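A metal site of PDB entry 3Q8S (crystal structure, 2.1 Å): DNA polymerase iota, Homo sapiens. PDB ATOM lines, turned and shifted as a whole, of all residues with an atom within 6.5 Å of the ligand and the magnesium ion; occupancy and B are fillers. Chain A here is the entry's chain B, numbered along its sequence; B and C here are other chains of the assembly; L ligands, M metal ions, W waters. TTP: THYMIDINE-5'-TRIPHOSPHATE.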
ATOM      1  N   ASP A  34       3.492 -22.019  31.821  1.00  0.00           N
ATOM      2  CA  ASP A  34       2.936 -20.784  31.289  1.00  0.00           C
ATOM      3  C   ASP A  34       2.959 -20.861  29.764  1.00  0.00           C
ATOM      4  O   ASP A  34       4.022 -20.846  29.156  1.00  0.00           O
ATOM      5  CB  ASP A  34       3.794 -19.595  31.763  1.00  0.00           C
ATOM      6  CG  ASP A  34       3.133 -18.260  31.481  1.00  0.00           C
ATOM      7  OD1 ASP A  34       2.267 -18.214  30.590  1.00  0.00           O
ATOM      8  OD2 ASP A  34       3.464 -17.260  32.141  1.00  0.00           O
ATOM      9  N   LEU A  35       1.774 -20.953  29.156  1.00  0.00           N
ATOM     10  CA  LEU A  35       1.690 -21.190  27.708  1.00  0.00           C
ATOM     11  C   LEU A  35       2.122 -19.976  26.922  1.00  0.00           C
ATOM     12  O   LEU A  35       1.904 -18.862  27.343  1.00  0.00           O
ATOM     13  CB  LEU A  35       0.249 -21.550  27.319  1.00  0.00           C
ATOM     14  CG  LEU A  35      -0.129 -23.018  27.387  1.00  0.00           C
ATOM     15  CD1 LEU A  35       0.535 -23.690  28.542  1.00  0.00           C
ATOM     16  CD2 LEU A  35      -1.649 -23.220  27.459  1.00  0.00           C
ATOM     17  N   ASP A  36       2.740 -20.197  25.770  1.00  0.00           N
ATOM     18  CA  ASP A  36       3.123 -19.089  24.917  1.00  0.00           C
ATOM     19  C   ASP A  36       2.089 -18.416  24.019  1.00  0.00           C
ATOM     20  O   ASP A  36       1.447 -19.080  23.193  1.00  0.00           O
ATOM     21  CB  ASP A  36       4.091 -19.563  23.824  1.00  0.00           C
ATOM     22  CG  ASP A  36       5.384 -20.120  24.389  1.00  0.00           C
ATOM     23  OD1 ASP A  36       5.886 -19.595  25.421  1.00  0.00           O
ATOM     24  OD2 ASP A  36       5.909 -21.071  23.801  1.00  0.00           O
ATOM     25  N   CYS A  37       1.933 -17.093  24.192  1.00  0.00           N
ATOM     26  CA  CYS A  37       0.865 -16.270  23.642  1.00  0.00           C
ATOM     27  C   CYS A  37      -0.452 -17.043  23.488  1.00  0.00           C
ATOM     28  O   CYS A  37      -0.954 -17.206  22.386  1.00  0.00           O
ATOM     29  CB  CYS A  37       1.313 -15.687  22.297  1.00  0.00           C
ATOM     30  SG  CYS A  37       1.925 -16.902  21.118  1.00  0.00           S
ATOM     31  N   PHE A  38      -1.011 -17.469  24.613  1.00  0.00           N
ATOM     32  CA  PHE A  38      -2.071 -18.482  24.630  1.00  0.00           C
ATOM     33  C   PHE A  38      -3.175 -18.356  23.554  1.00  0.00           C
ATOM     34  O   PHE A  38      -3.309 -19.236  22.716  1.00  0.00           O
ATOM     35  CB  PHE A  38      -2.707 -18.613  26.013  1.00  0.00           C
ATOM     36  CG  PHE A  38      -3.706 -19.735  26.104  1.00  0.00           C
ATOM     37  CD1 PHE A  38      -3.391 -20.993  25.627  1.00  0.00           C
ATOM     38  CD2 PHE A  38      -4.950 -19.527  26.664  1.00  0.00           C
ATOM     39  CE1 PHE A  38      -4.313 -22.037  25.699  1.00  0.00           C
ATOM     40  CE2 PHE A  38      -5.868 -20.557  26.745  1.00  0.00           C
ATOM     41  CZ  PHE A  38      -5.545 -21.813  26.274  1.00  0.00           C
ATOM     42  N   TYR A  39      -3.963 -17.284  23.604  1.00  0.00           N
ATOM     43  CA  TYR A  39      -5.087 -17.148  22.658  1.00  0.00           C
ATOM     44  C   TYR A  39      -4.600 -17.236  21.214  1.00  0.00           C
ATOM     45  O   TYR A  39      -5.159 -17.970  20.406  1.00  0.00           O
ATOM     46  CB  TYR A  39      -5.826 -15.822  22.851  1.00  0.00           C
ATOM     47  CG  TYR A  39      -6.633 -15.715  24.116  1.00  0.00           C
ATOM     48  CD1 TYR A  39      -7.386 -14.572  24.363  1.00  0.00           C
ATOM     49  CD2 TYR A  39      -6.621 -16.714  25.087  1.00  0.00           C
ATOM     50  CE1 TYR A  39      -8.136 -14.447  25.528  1.00  0.00           C
ATOM     51  CE2 TYR A  39      -7.364 -16.596  26.262  1.00  0.00           C
ATOM     52  CZ  TYR A  39      -8.113 -15.448  26.468  1.00  0.00           C
ATOM     53  OH  TYR A  39      -8.853 -15.299  27.614  1.00  0.00           O
ATOM     54  N   ALA A  40      -3.548 -16.484  20.912  1.00  0.00           N
ATOM     55  CA  ALA A  40      -2.979 -16.467  19.575  1.00  0.00           C
ATOM     56  C   ALA A  40      -2.542 -17.875  19.145  1.00  0.00           C
ATOM     57  O   ALA A  40      -2.750 -18.267  18.005  1.00  0.00           O
ATOM     58  CB  ALA A  40      -1.812 -15.497  19.486  1.00  0.00           C
ATOM     59  N   GLN A  59     -10.345  -8.028  21.174  1.00  0.00           N
ATOM     60  CA  GLN A  59     -11.569  -7.999  21.948  1.00  0.00           C
ATOM     61  C   GLN A  59     -12.041  -6.548  22.001  1.00  0.00           C
ATOM     62  O   GLN A  59     -11.424  -5.706  22.637  1.00  0.00           O
ATOM     63  CB  GLN A  59     -11.325  -8.556  23.358  1.00  0.00           C
ATOM     64  CG  GLN A  59     -11.128 -10.069  23.406  1.00  0.00           C
ATOM     65  CD  GLN A  59     -10.796 -10.578  24.806  1.00  0.00           C
ATOM     66  OE1 GLN A  59     -10.323  -9.821  25.644  1.00  0.00           O
ATOM     67  NE2 GLN A  59     -11.055 -11.863  25.053  1.00  0.00           N
ATOM     68  N   VAL A  64      -5.693  -8.053  22.956  1.00  0.00           N
ATOM     69  CA  VAL A  64      -5.392  -8.629  24.256  1.00  0.00           C
ATOM     70  C   VAL A  64      -4.048  -9.346  24.260  1.00  0.00           C
ATOM     71  O   VAL A  64      -3.311  -9.284  25.242  1.00  0.00           O
ATOM     72  CB  VAL A  64      -6.523  -9.547  24.770  1.00  0.00           C
ATOM     73  CG1 VAL A  64      -7.812  -8.777  24.783  1.00  0.00           C
ATOM     74  CG2 VAL A  64      -6.663 -10.803  23.909  1.00  0.00           C
ATOM     75  N   THR A  65      -3.730 -10.012  23.163  1.00  0.00           N
ATOM     76  CA  THR A  65      -2.433 -10.654  23.010  1.00  0.00           C
ATOM     77  C   THR A  65      -2.100 -10.845  21.525  1.00  0.00           C
ATOM     78  O   THR A  65      -2.966 -10.700  20.666  1.00  0.00           O
ATOM     79  CB  THR A  65      -2.371 -12.023  23.741  1.00  0.00           C
ATOM     80  OG1 THR A  65      -1.011 -12.450  23.858  1.00  0.00           O
ATOM     81  CG2 THR A  65      -3.178 -13.090  23.015  1.00  0.00           C
ATOM     82  N   CYS A  66      -0.844 -11.162  21.246  1.00  0.00           N
ATOM     83  CA  CYS A  66      -0.371 -11.370  19.879  1.00  0.00           C
ATOM     84  C   CYS A  66       0.738 -12.414  19.876  1.00  0.00           C
ATOM     85  O   CYS A  66       1.386 -12.627  20.897  1.00  0.00           O
ATOM     86  CB  CYS A  66       0.154 -10.054  19.306  1.00  0.00           C
ATOM     87  SG  CYS A  66       1.470  -9.282  20.292  1.00  0.00           S
ATOM     88  N   TYR A  68       4.473 -14.143  18.612  1.00  0.00           N
ATOM     89  CA  TYR A  68       5.819 -13.583  18.731  1.00  0.00           C
ATOM     90  C   TYR A  68       6.326 -12.951  17.449  1.00  0.00           C
ATOM     91  O   TYR A  68       7.235 -12.118  17.472  1.00  0.00           O
ATOM     92  CB  TYR A  68       6.792 -14.623  19.301  1.00  0.00           C
ATOM     93  CG  TYR A  68       6.624 -14.756  20.791  1.00  0.00           C
ATOM     94  CD1 TYR A  68       5.621 -15.544  21.326  1.00  0.00           C
ATOM     95  CD2 TYR A  68       7.458 -14.066  21.672  1.00  0.00           C
ATOM     96  CE1 TYR A  68       5.442 -15.660  22.690  1.00  0.00           C
ATOM     97  CE2 TYR A  68       7.297 -14.170  23.044  1.00  0.00           C
ATOM     98  CZ  TYR A  68       6.293 -14.980  23.549  1.00  0.00           C
ATOM     99  OH  TYR A  68       6.107 -15.097  24.907  1.00  0.00           O
ATOM    100  N   ARG A  71       5.123  -9.414  18.127  1.00  0.00           N
ATOM    101  CA  ARG A  71       5.865  -8.678  19.146  1.00  0.00           C
ATOM    102  C   ARG A  71       7.198  -8.215  18.593  1.00  0.00           C
ATOM    103  O   ARG A  71       7.737  -7.188  19.008  1.00  0.00           O
ATOM    104  CB  ARG A  71       6.059  -9.536  20.407  1.00  0.00           C
ATOM    105  CG  ARG A  71       4.748 -10.028  21.004  1.00  0.00           C
ATOM    106  CD  ARG A  71       4.939 -10.863  22.266  1.00  0.00           C
ATOM    107  NE  ARG A  71       3.708 -11.560  22.618  1.00  0.00           N
ATOM    108  CZ  ARG A  71       3.493 -12.181  23.782  1.00  0.00           C
ATOM    109  NH1 ARG A  71       4.435 -12.198  24.718  1.00  0.00           N
ATOM    110  NH2 ARG A  71       2.335 -12.789  23.998  1.00  0.00           N
ATOM    111  N   LYS A  77       1.159  -6.616  24.339  1.00  0.00           N
ATOM    112  CA  LYS A  77      -0.076  -7.130  24.938  1.00  0.00           C
ATOM    113  C   LYS A  77      -0.981  -5.987  25.380  1.00  0.00           C
ATOM    114  O   LYS A  77      -0.526  -4.987  25.919  1.00  0.00           O
ATOM    115  CB  LYS A  77       0.227  -8.025  26.140  1.00  0.00           C
ATOM    116  CG  LYS A  77       1.040  -9.263  25.810  1.00  0.00           C
ATOM    117  CD  LYS A  77       1.092 -10.194  27.025  1.00  0.00           C
ATOM    118  CE  LYS A  77       2.520 -10.622  27.358  1.00  0.00           C
ATOM    119  NZ  LYS A  77       2.565 -11.446  28.596  1.00  0.00           N
ATOM    120  N   LEU A  78      -2.289  -6.153  25.149  1.00  0.00           N
ATOM    121  CA  LEU A  78      -3.281  -5.186  25.609  1.00  0.00           C
ATOM    122  C   LEU A  78      -3.145  -3.807  24.946  1.00  0.00           C
ATOM    123  O   LEU A  78      -3.544  -2.797  25.536  1.00  0.00           O
ATOM    124  CB  LEU A  78      -3.226  -5.035  27.131  1.00  0.00           C
ATOM    125  CG  LEU A  78      -3.433  -6.307  27.959  1.00  0.00           C
ATOM    126  CD1 LEU A  78      -2.860  -6.136  29.358  1.00  0.00           C
ATOM    127  CD2 LEU A  78      -4.898  -6.683  28.023  1.00  0.00           C
ATOM    128  N   LEU A  99     -14.707 -16.921  24.472  1.00  0.00           N
ATOM    129  CA  LEU A  99     -13.595 -17.626  25.093  1.00  0.00           C
ATOM    130  C   LEU A  99     -13.725 -19.143  25.011  1.00  0.00           C
ATOM    131  O   LEU A  99     -12.883 -19.859  25.562  1.00  0.00           O
ATOM    132  CB  LEU A  99     -13.475 -17.244  26.565  1.00  0.00           C
ATOM    133  CG  LEU A  99     -13.256 -15.770  26.929  1.00  0.00           C
ATOM    134  CD1 LEU A  99     -12.817 -15.654  28.387  1.00  0.00           C
ATOM    135  CD2 LEU A  99     -12.238 -15.136  26.004  1.00  0.00           C
ATOM    136  N   PHE A 125      -6.360 -18.732  32.488  1.00  0.00           N
ATOM    137  CA  PHE A 125      -6.579 -19.786  31.507  1.00  0.00           C
ATOM    138  C   PHE A 125      -5.320 -20.481  31.037  1.00  0.00           C
ATOM    139  O   PHE A 125      -5.390 -21.585  30.482  1.00  0.00           O
ATOM    140  CB  PHE A 125      -7.350 -19.264  30.288  1.00  0.00           C
ATOM    141  CG  PHE A 125      -8.839 -19.210  30.475  1.00  0.00           C
ATOM    142  CD1 PHE A 125      -9.405 -19.430  31.710  1.00  0.00           C
ATOM    143  CD2 PHE A 125      -9.686 -18.948  29.395  1.00  0.00           C
ATOM    144  CE1 PHE A 125     -10.778 -19.373  31.890  1.00  0.00           C
ATOM    145  CE2 PHE A 125     -11.047 -18.898  29.561  1.00  0.00           C
ATOM    146  CZ  PHE A 125     -11.598 -19.116  30.807  1.00  0.00           C
ATOM    147  N   ASP A 126      -4.164 -19.858  31.221  1.00  0.00           N
ATOM    148  CA  ASP A 126      -2.981 -20.431  30.591  1.00  0.00           C
ATOM    149  C   ASP A 126      -1.796 -20.734  31.519  1.00  0.00           C
ATOM    150  O   ASP A 126      -0.708 -21.051  31.041  1.00  0.00           O
ATOM    151  CB  ASP A 126      -2.526 -19.563  29.423  1.00  0.00           C
ATOM    152  CG  ASP A 126      -1.422 -18.596  29.805  1.00  0.00           C
ATOM    153  OD1 ASP A 126      -0.407 -18.574  29.088  1.00  0.00           O
ATOM    154  OD2 ASP A 126      -1.574 -17.879  30.815  1.00  0.00           O
ATOM    155  N   GLU A 127      -2.007 -20.674  32.824  1.00  0.00           N
ATOM    156  CA  GLU A 127      -0.933 -20.997  33.771  1.00  0.00           C
ATOM    157  C   GLU A 127      -1.364 -22.064  34.770  1.00  0.00           C
ATOM    158  O   GLU A 127      -2.516 -22.090  35.177  1.00  0.00           O
ATOM    159  CB  GLU A 127      -0.460 -19.747  34.513  1.00  0.00           C
ATOM    160  CG  GLU A 127       0.286 -18.768  33.627  1.00  0.00           C
ATOM    161  CD  GLU A 127       0.527 -17.438  34.298  1.00  0.00           C
ATOM    162  OE1 GLU A 127       0.812 -17.433  35.527  1.00  0.00           O
ATOM    163  OE2 GLU A 127       0.439 -16.402  33.617  1.00  0.00           O
ATOM    164  N   LYS A 214      12.019 -16.826  27.242  1.00  0.00           N
ATOM    165  CA  LYS A 214      10.787 -16.996  26.472  1.00  0.00           C
ATOM    166  C   LYS A 214      11.081 -16.741  25.007  1.00  0.00           C
ATOM    167  O   LYS A 214      12.012 -16.011  24.689  1.00  0.00           O
ATOM    168  CB  LYS A 214       9.738 -15.973  26.915  1.00  0.00           C
ATOM    169  CG  LYS A 214       9.023 -16.318  28.191  1.00  0.00           C
ATOM    170  CD  LYS A 214       8.356 -15.075  28.782  1.00  0.00           C
ATOM    171  CE  LYS A 214       7.493 -14.373  27.744  1.00  0.00           C
ATOM    172  NZ  LYS A 214       6.610 -13.332  28.348  1.00  0.00           N
ATOM    173  N   PRO A 215      10.278 -17.328  24.098  1.00  0.00           N
ATOM    174  CA  PRO A 215       9.180 -18.253  24.410  1.00  0.00           C
ATOM    175  C   PRO A 215       9.646 -19.714  24.384  1.00  0.00           C
ATOM    176  O   PRO A 215      10.793 -19.996  24.044  1.00  0.00           O
ATOM    177  CB  PRO A 215       8.192 -18.015  23.273  1.00  0.00           C
ATOM    178  CG  PRO A 215       9.050 -17.669  22.108  1.00  0.00           C
ATOM    179  CD  PRO A 215      10.257 -16.923  22.680  1.00  0.00           C
ATOM    180  P   8OG B   4     -13.951  -2.575  28.279  1.00  0.00           P
ATOM    181  OP1 8OG B   4     -15.102  -1.741  27.809  1.00  0.00           O
ATOM    182  OP2 8OG B   4     -12.617  -1.914  28.569  1.00  0.00           O
ATOM    183  O5' 8OG B   4     -13.715  -3.740  27.203  1.00  0.00           O
ATOM    184  C5' 8OG B   4     -12.390  -4.201  26.941  1.00  0.00           C
ATOM    185  C4' 8OG B   4     -12.392  -5.657  26.479  1.00  0.00           C
ATOM    186  O4' 8OG B   4     -11.143  -6.237  26.831  1.00  0.00           O
ATOM    187  C3' 8OG B   4     -13.496  -6.500  27.113  1.00  0.00           C
ATOM    188  O3' 8OG B   4     -14.091  -7.287  26.071  1.00  0.00           O
ATOM    189  C2' 8OG B   4     -12.770  -7.407  28.105  1.00  0.00           C
ATOM    190  C1' 8OG B   4     -11.296  -7.340  27.725  1.00  0.00           C
ATOM    191  N9  8OG B   4     -10.346  -7.244  28.870  1.00  0.00           N
ATOM    192  C8  8OG B   4      -9.261  -8.000  29.072  1.00  0.00           C
ATOM    193  N7  8OG B   4      -8.537  -7.755  30.157  1.00  0.00           N
ATOM    194  C5  8OG B   4      -9.181  -6.730  30.725  1.00  0.00           C
ATOM    195  C6  8OG B   4      -8.953  -5.929  31.949  1.00  0.00           C
ATOM    196  O6  8OG B   4      -7.978  -6.184  32.675  1.00  0.00           O
ATOM    197  N1  8OG B   4      -9.820  -4.952  32.230  1.00  0.00           N
ATOM    198  C2  8OG B   4     -10.878  -4.676  31.443  1.00  0.00           C
ATOM    199  N2  8OG B   4     -11.697  -3.652  31.806  1.00  0.00           N
ATOM    200  N3  8OG B   4     -11.147  -5.362  30.306  1.00  0.00           N
ATOM    201  C4  8OG B   4     -10.355  -6.390  29.896  1.00  0.00           C
ATOM    202  O8  8OG B   4      -8.941  -8.929  28.299  1.00  0.00           O
ATOM    203  P    DG B   5     -15.520  -8.005  26.185  1.00  0.00           P
ATOM    204  OP1  DG B   5     -16.042  -8.422  24.866  1.00  0.00           O
ATOM    205  OP2  DG B   5     -16.324  -7.213  27.125  1.00  0.00           O
ATOM    206  O5'  DG B   5     -15.059  -9.354  26.890  1.00  0.00           O
ATOM    207  C5'  DG B   5     -14.599 -10.485  26.150  1.00  0.00           C
ATOM    208  C4'  DG B   5     -14.273 -11.620  27.106  1.00  0.00           C
ATOM    209  O4'  DG B   5     -13.193 -11.197  27.972  1.00  0.00           O
ATOM    210  C3'  DG B   5     -15.419 -11.978  28.053  1.00  0.00           C
ATOM    211  O3'  DG B   5     -15.419 -13.358  28.318  1.00  0.00           O
ATOM    212  C2'  DG B   5     -15.091 -11.209  29.317  1.00  0.00           C
ATOM    213  C1'  DG B   5     -13.583 -11.451  29.294  1.00  0.00           C
ATOM    214  N9   DG B   5     -12.828 -10.618  30.206  1.00  0.00           N
ATOM    215  C8   DG B   5     -13.136  -9.369  30.693  1.00  0.00           C
ATOM    216  N7   DG B   5     -12.233  -8.903  31.521  1.00  0.00           N
ATOM    217  C5   DG B   5     -11.271  -9.910  31.561  1.00  0.00           C
ATOM    218  C6   DG B   5     -10.059  -9.973  32.282  1.00  0.00           C
ATOM    219  O6   DG B   5      -9.571  -9.127  33.047  1.00  0.00           O
ATOM    220  N1   DG B   5      -9.403 -11.175  32.044  1.00  0.00           N
ATOM    221  C2   DG B   5      -9.840 -12.180  31.221  1.00  0.00           C
ATOM    222  N2   DG B   5      -9.045 -13.268  31.130  1.00  0.00           N
ATOM    223  N3   DG B   5     -10.963 -12.127  30.534  1.00  0.00           N
ATOM    224  C4   DG B   5     -11.621 -10.970  30.766  1.00  0.00           C
ATOM    225  P    DC C   7      -0.488 -12.214  36.710  1.00  0.00           P
ATOM    226  OP1  DC C   7       0.919 -12.591  36.526  1.00  0.00           O
ATOM    227  OP2  DC C   7      -0.921 -10.790  36.766  1.00  0.00           O
ATOM    228  O5'  DC C   7      -1.366 -12.877  35.522  1.00  0.00           O
ATOM    229  C5'  DC C   7      -1.337 -14.294  35.337  1.00  0.00           C
ATOM    230  C4'  DC C   7      -2.344 -14.715  34.282  1.00  0.00           C
ATOM    231  O4'  DC C   7      -3.696 -14.553  34.794  1.00  0.00           O
ATOM    232  C3'  DC C   7      -2.344 -13.893  32.999  1.00  0.00           C
ATOM    233  C2'  DC C   7      -3.744 -14.210  32.458  1.00  0.00           C
ATOM    234  C1'  DC C   7      -4.562 -14.212  33.743  1.00  0.00           C
ATOM    235  N1   DC C   7      -5.192 -12.885  34.007  1.00  0.00           N
ATOM    236  C2   DC C   7      -6.390 -12.626  33.350  1.00  0.00           C
ATOM    237  O2   DC C   7      -6.845 -13.508  32.615  1.00  0.00           O
ATOM    238  N3   DC C   7      -7.003 -11.436  33.546  1.00  0.00           N
ATOM    239  C4   DC C   7      -6.436 -10.548  34.366  1.00  0.00           C
ATOM    240  N4   DC C   7      -7.062  -9.378  34.533  1.00  0.00           N
ATOM    241  C5   DC C   7      -5.212 -10.795  35.036  1.00  0.00           C
ATOM    242  C6   DC C   7      -4.620 -11.974  34.832  1.00  0.00           C
HETATM  243  PA  TTP L   1      -0.460 -14.055  29.698  1.00  0.00           P
HETATM  244  O1A TTP L   1      -0.217 -12.948  30.687  1.00  0.00           O
HETATM  245  O2A TTP L   1       0.031 -15.367  30.232  1.00  0.00           O
HETATM  246  O3A TTP L   1       0.247 -13.715  28.296  1.00  0.00           O
HETATM  247  PB  TTP L   1       0.234 -14.688  27.011  1.00  0.00           P
HETATM  248  O1B TTP L   1       0.082 -16.135  27.381  1.00  0.00           O
HETATM  249  O2B TTP L   1      -0.862 -14.250  26.072  1.00  0.00           O
HETATM  250  O3B TTP L   1       1.644 -14.416  26.300  1.00  0.00           O
HETATM  251  PG  TTP L   1       3.054 -14.821  26.965  1.00  0.00           P
HETATM  252  O1G TTP L   1       3.848 -15.587  25.948  1.00  0.00           O
HETATM  253  O2G TTP L   1       2.859 -15.657  28.196  1.00  0.00           O
HETATM  254  O3G TTP L   1       3.769 -13.552  27.314  1.00  0.00           O
HETATM  255  O5' TTP L   1      -2.034 -14.141  29.356  1.00  0.00           O
HETATM  256  C5' TTP L   1      -2.662 -15.393  29.108  1.00  0.00           C
HETATM  257  C4' TTP L   1      -3.940 -15.167  28.309  1.00  0.00           C
HETATM  258  O4' TTP L   1      -4.931 -14.527  29.124  1.00  0.00           O
HETATM  259  C3' TTP L   1      -3.689 -14.256  27.124  1.00  0.00           C
HETATM  260  O3' TTP L   1      -3.640 -15.023  25.921  1.00  0.00           O
HETATM  261  C2' TTP L   1      -4.843 -13.281  27.099  1.00  0.00           C
HETATM  262  C1' TTP L   1      -5.607 -13.507  28.387  1.00  0.00           C
HETATM  263  N1  TTP L   1      -5.675 -12.252  29.141  1.00  0.00           N
HETATM  264  C2  TTP L   1      -6.837 -11.455  29.075  1.00  0.00           C
HETATM  265  O2  TTP L   1      -7.799 -11.844  28.367  1.00  0.00           O
HETATM  266  N3  TTP L   1      -6.939 -10.295  29.740  1.00  0.00           N
HETATM  267  C4  TTP L   1      -5.929  -9.863  30.493  1.00  0.00           C
HETATM  268  O4  TTP L   1      -6.014  -8.786  31.116  1.00  0.00           O
HETATM  269  C5  TTP L   1      -4.700 -10.679  30.591  1.00  0.00           C
HETATM  270  C5M TTP L   1      -3.554 -10.196  31.439  1.00  0.00           C
HETATM  271  C6  TTP L   1      -4.630 -11.870  29.890  1.00  0.00           C
HETATM  272 MG    MG M   1       1.391 -17.255  28.758  1.00  0.00          MG
HETATM  273  O   HOH W   1     -10.127 -13.020  27.923  1.00  0.00           O
HETATM  274  O   HOH W   2       1.136 -12.427  32.795  1.00  0.00           O
HETATM  275  O   HOH W   3       4.182 -18.161  28.884  1.00  0.00           O
HETATM  276  O   HOH W   4       3.615 -14.673  30.862  1.00  0.00           O
HETATM  277  O   HOH W   5      -3.731  -7.645  33.206  1.00  0.00           O
HETATM  278  O   HOH W   6       5.846 -17.332  26.635  1.00  0.00           O
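OH of Tyr 68 sits at hydrogen-bond distance from O1G of the ligand.
The side-chain amino group (NZ) of Lys 77 is in salt-bridge range of an oxygen (O3G) of the ligand (2.7 Å).
O8 of 8OG 4 of chain B lies within hydrogen-bond range of a nitrogen (N3) of the ligand (2.8 Å).
An oxygen (O2B) of the ligand is in hydrogen-bond range of the side-chain hydroxyl (OG1) of Thr 65, at 2.9 Å.
NH1 of Arg 71 is in salt-bridge range of O3G of the ligand, at 3.0 Å.
N of Cys 37 sits at hydrogen-bond distance from O1G of the ligand, 3.0 Å away.
O3G of the ligand is in salt-bridge range of NZ of Lys 214 (3.0 Å).
The backbone NH (N) of Tyr 39 lies within hydrogen-bond range of an oxygen (O3') of the ligand, 3.3 Å away.
N of Phe 38 lies close to O1B of the ligand, at 3.3 Å.
N1 of DG 5 of chain B is in hydrogen-bond range of a nitrogen (N3) of the ligand (3.5 Å).
NH1 of Arg 71 sits at hydrogen-bond distance from OH of Tyr 68, 3.4 Å away.
O8 of 8OG 4 of chain B lies close to the side-chain amide oxygen (OE1) of Gln 59, 3.1 Å away.
NH2 of Arg 71 sits at hydrogen-bond distance from OG1 of Thr 65, at 3.4 Å.
O of Cys 66 is in hydrogen-bond range of NE of Arg 71 (3.1 Å).
O2 of DC 7 of chain C lies close to N2 of DG 5 of chain B.
The backbone carbonyl oxygen of Val 64 sits at hydrogen-bond distance from the backbone NH of Leu 78, 3.3 Å away.
Merely in contact with the ligand: DC 7 of chain C (3.3 Å), Glu 127 (3.6 Å), Asp 36 (3.7 Å) and Leu 78 (3.9 Å).
Hydrophobic or aromatic side chains within 4 Å of the ligand: Phe 38, Tyr 39, Tyr 68 and Leu 78.
Of the 24 residues printed, 3 come within 4 Å of the magnesium ion.
Along chain A the residues within 4 Å of the magnesium ion span positions 34 to 126.
The nearest printed residue that does not touch the magnesium ion is Asp 36 (4.4 Å).
The magnesium ion is bound by the backbone carbonyl oxygen (O) of Leu 35 (2.2 Å).
An oxygen (O1B) of the ligand is bound to the magnesium ion.
O2G of the ligand binds the magnesium ion (2.2 Å).
The magnesium ion is bound by the side-chain carboxylate (OD1) of Asp 34, at 2.2 Å.
OD1 of Asp 126 is bound to the magnesium ion, at 2.3 Å.
Slightly farther from the magnesium ion lies O2A of the ligand (2.8 Å).
Water W1 lies within hydrogen-bond range of OH of Tyr 39, O2 of the ligand, N3 of DG 5 of chain B and NE2 of Gln 59.
Water W6 lies within hydrogen-bond range of OD1 of Asp 36, O1G of the ligand and OH of Tyr 68.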
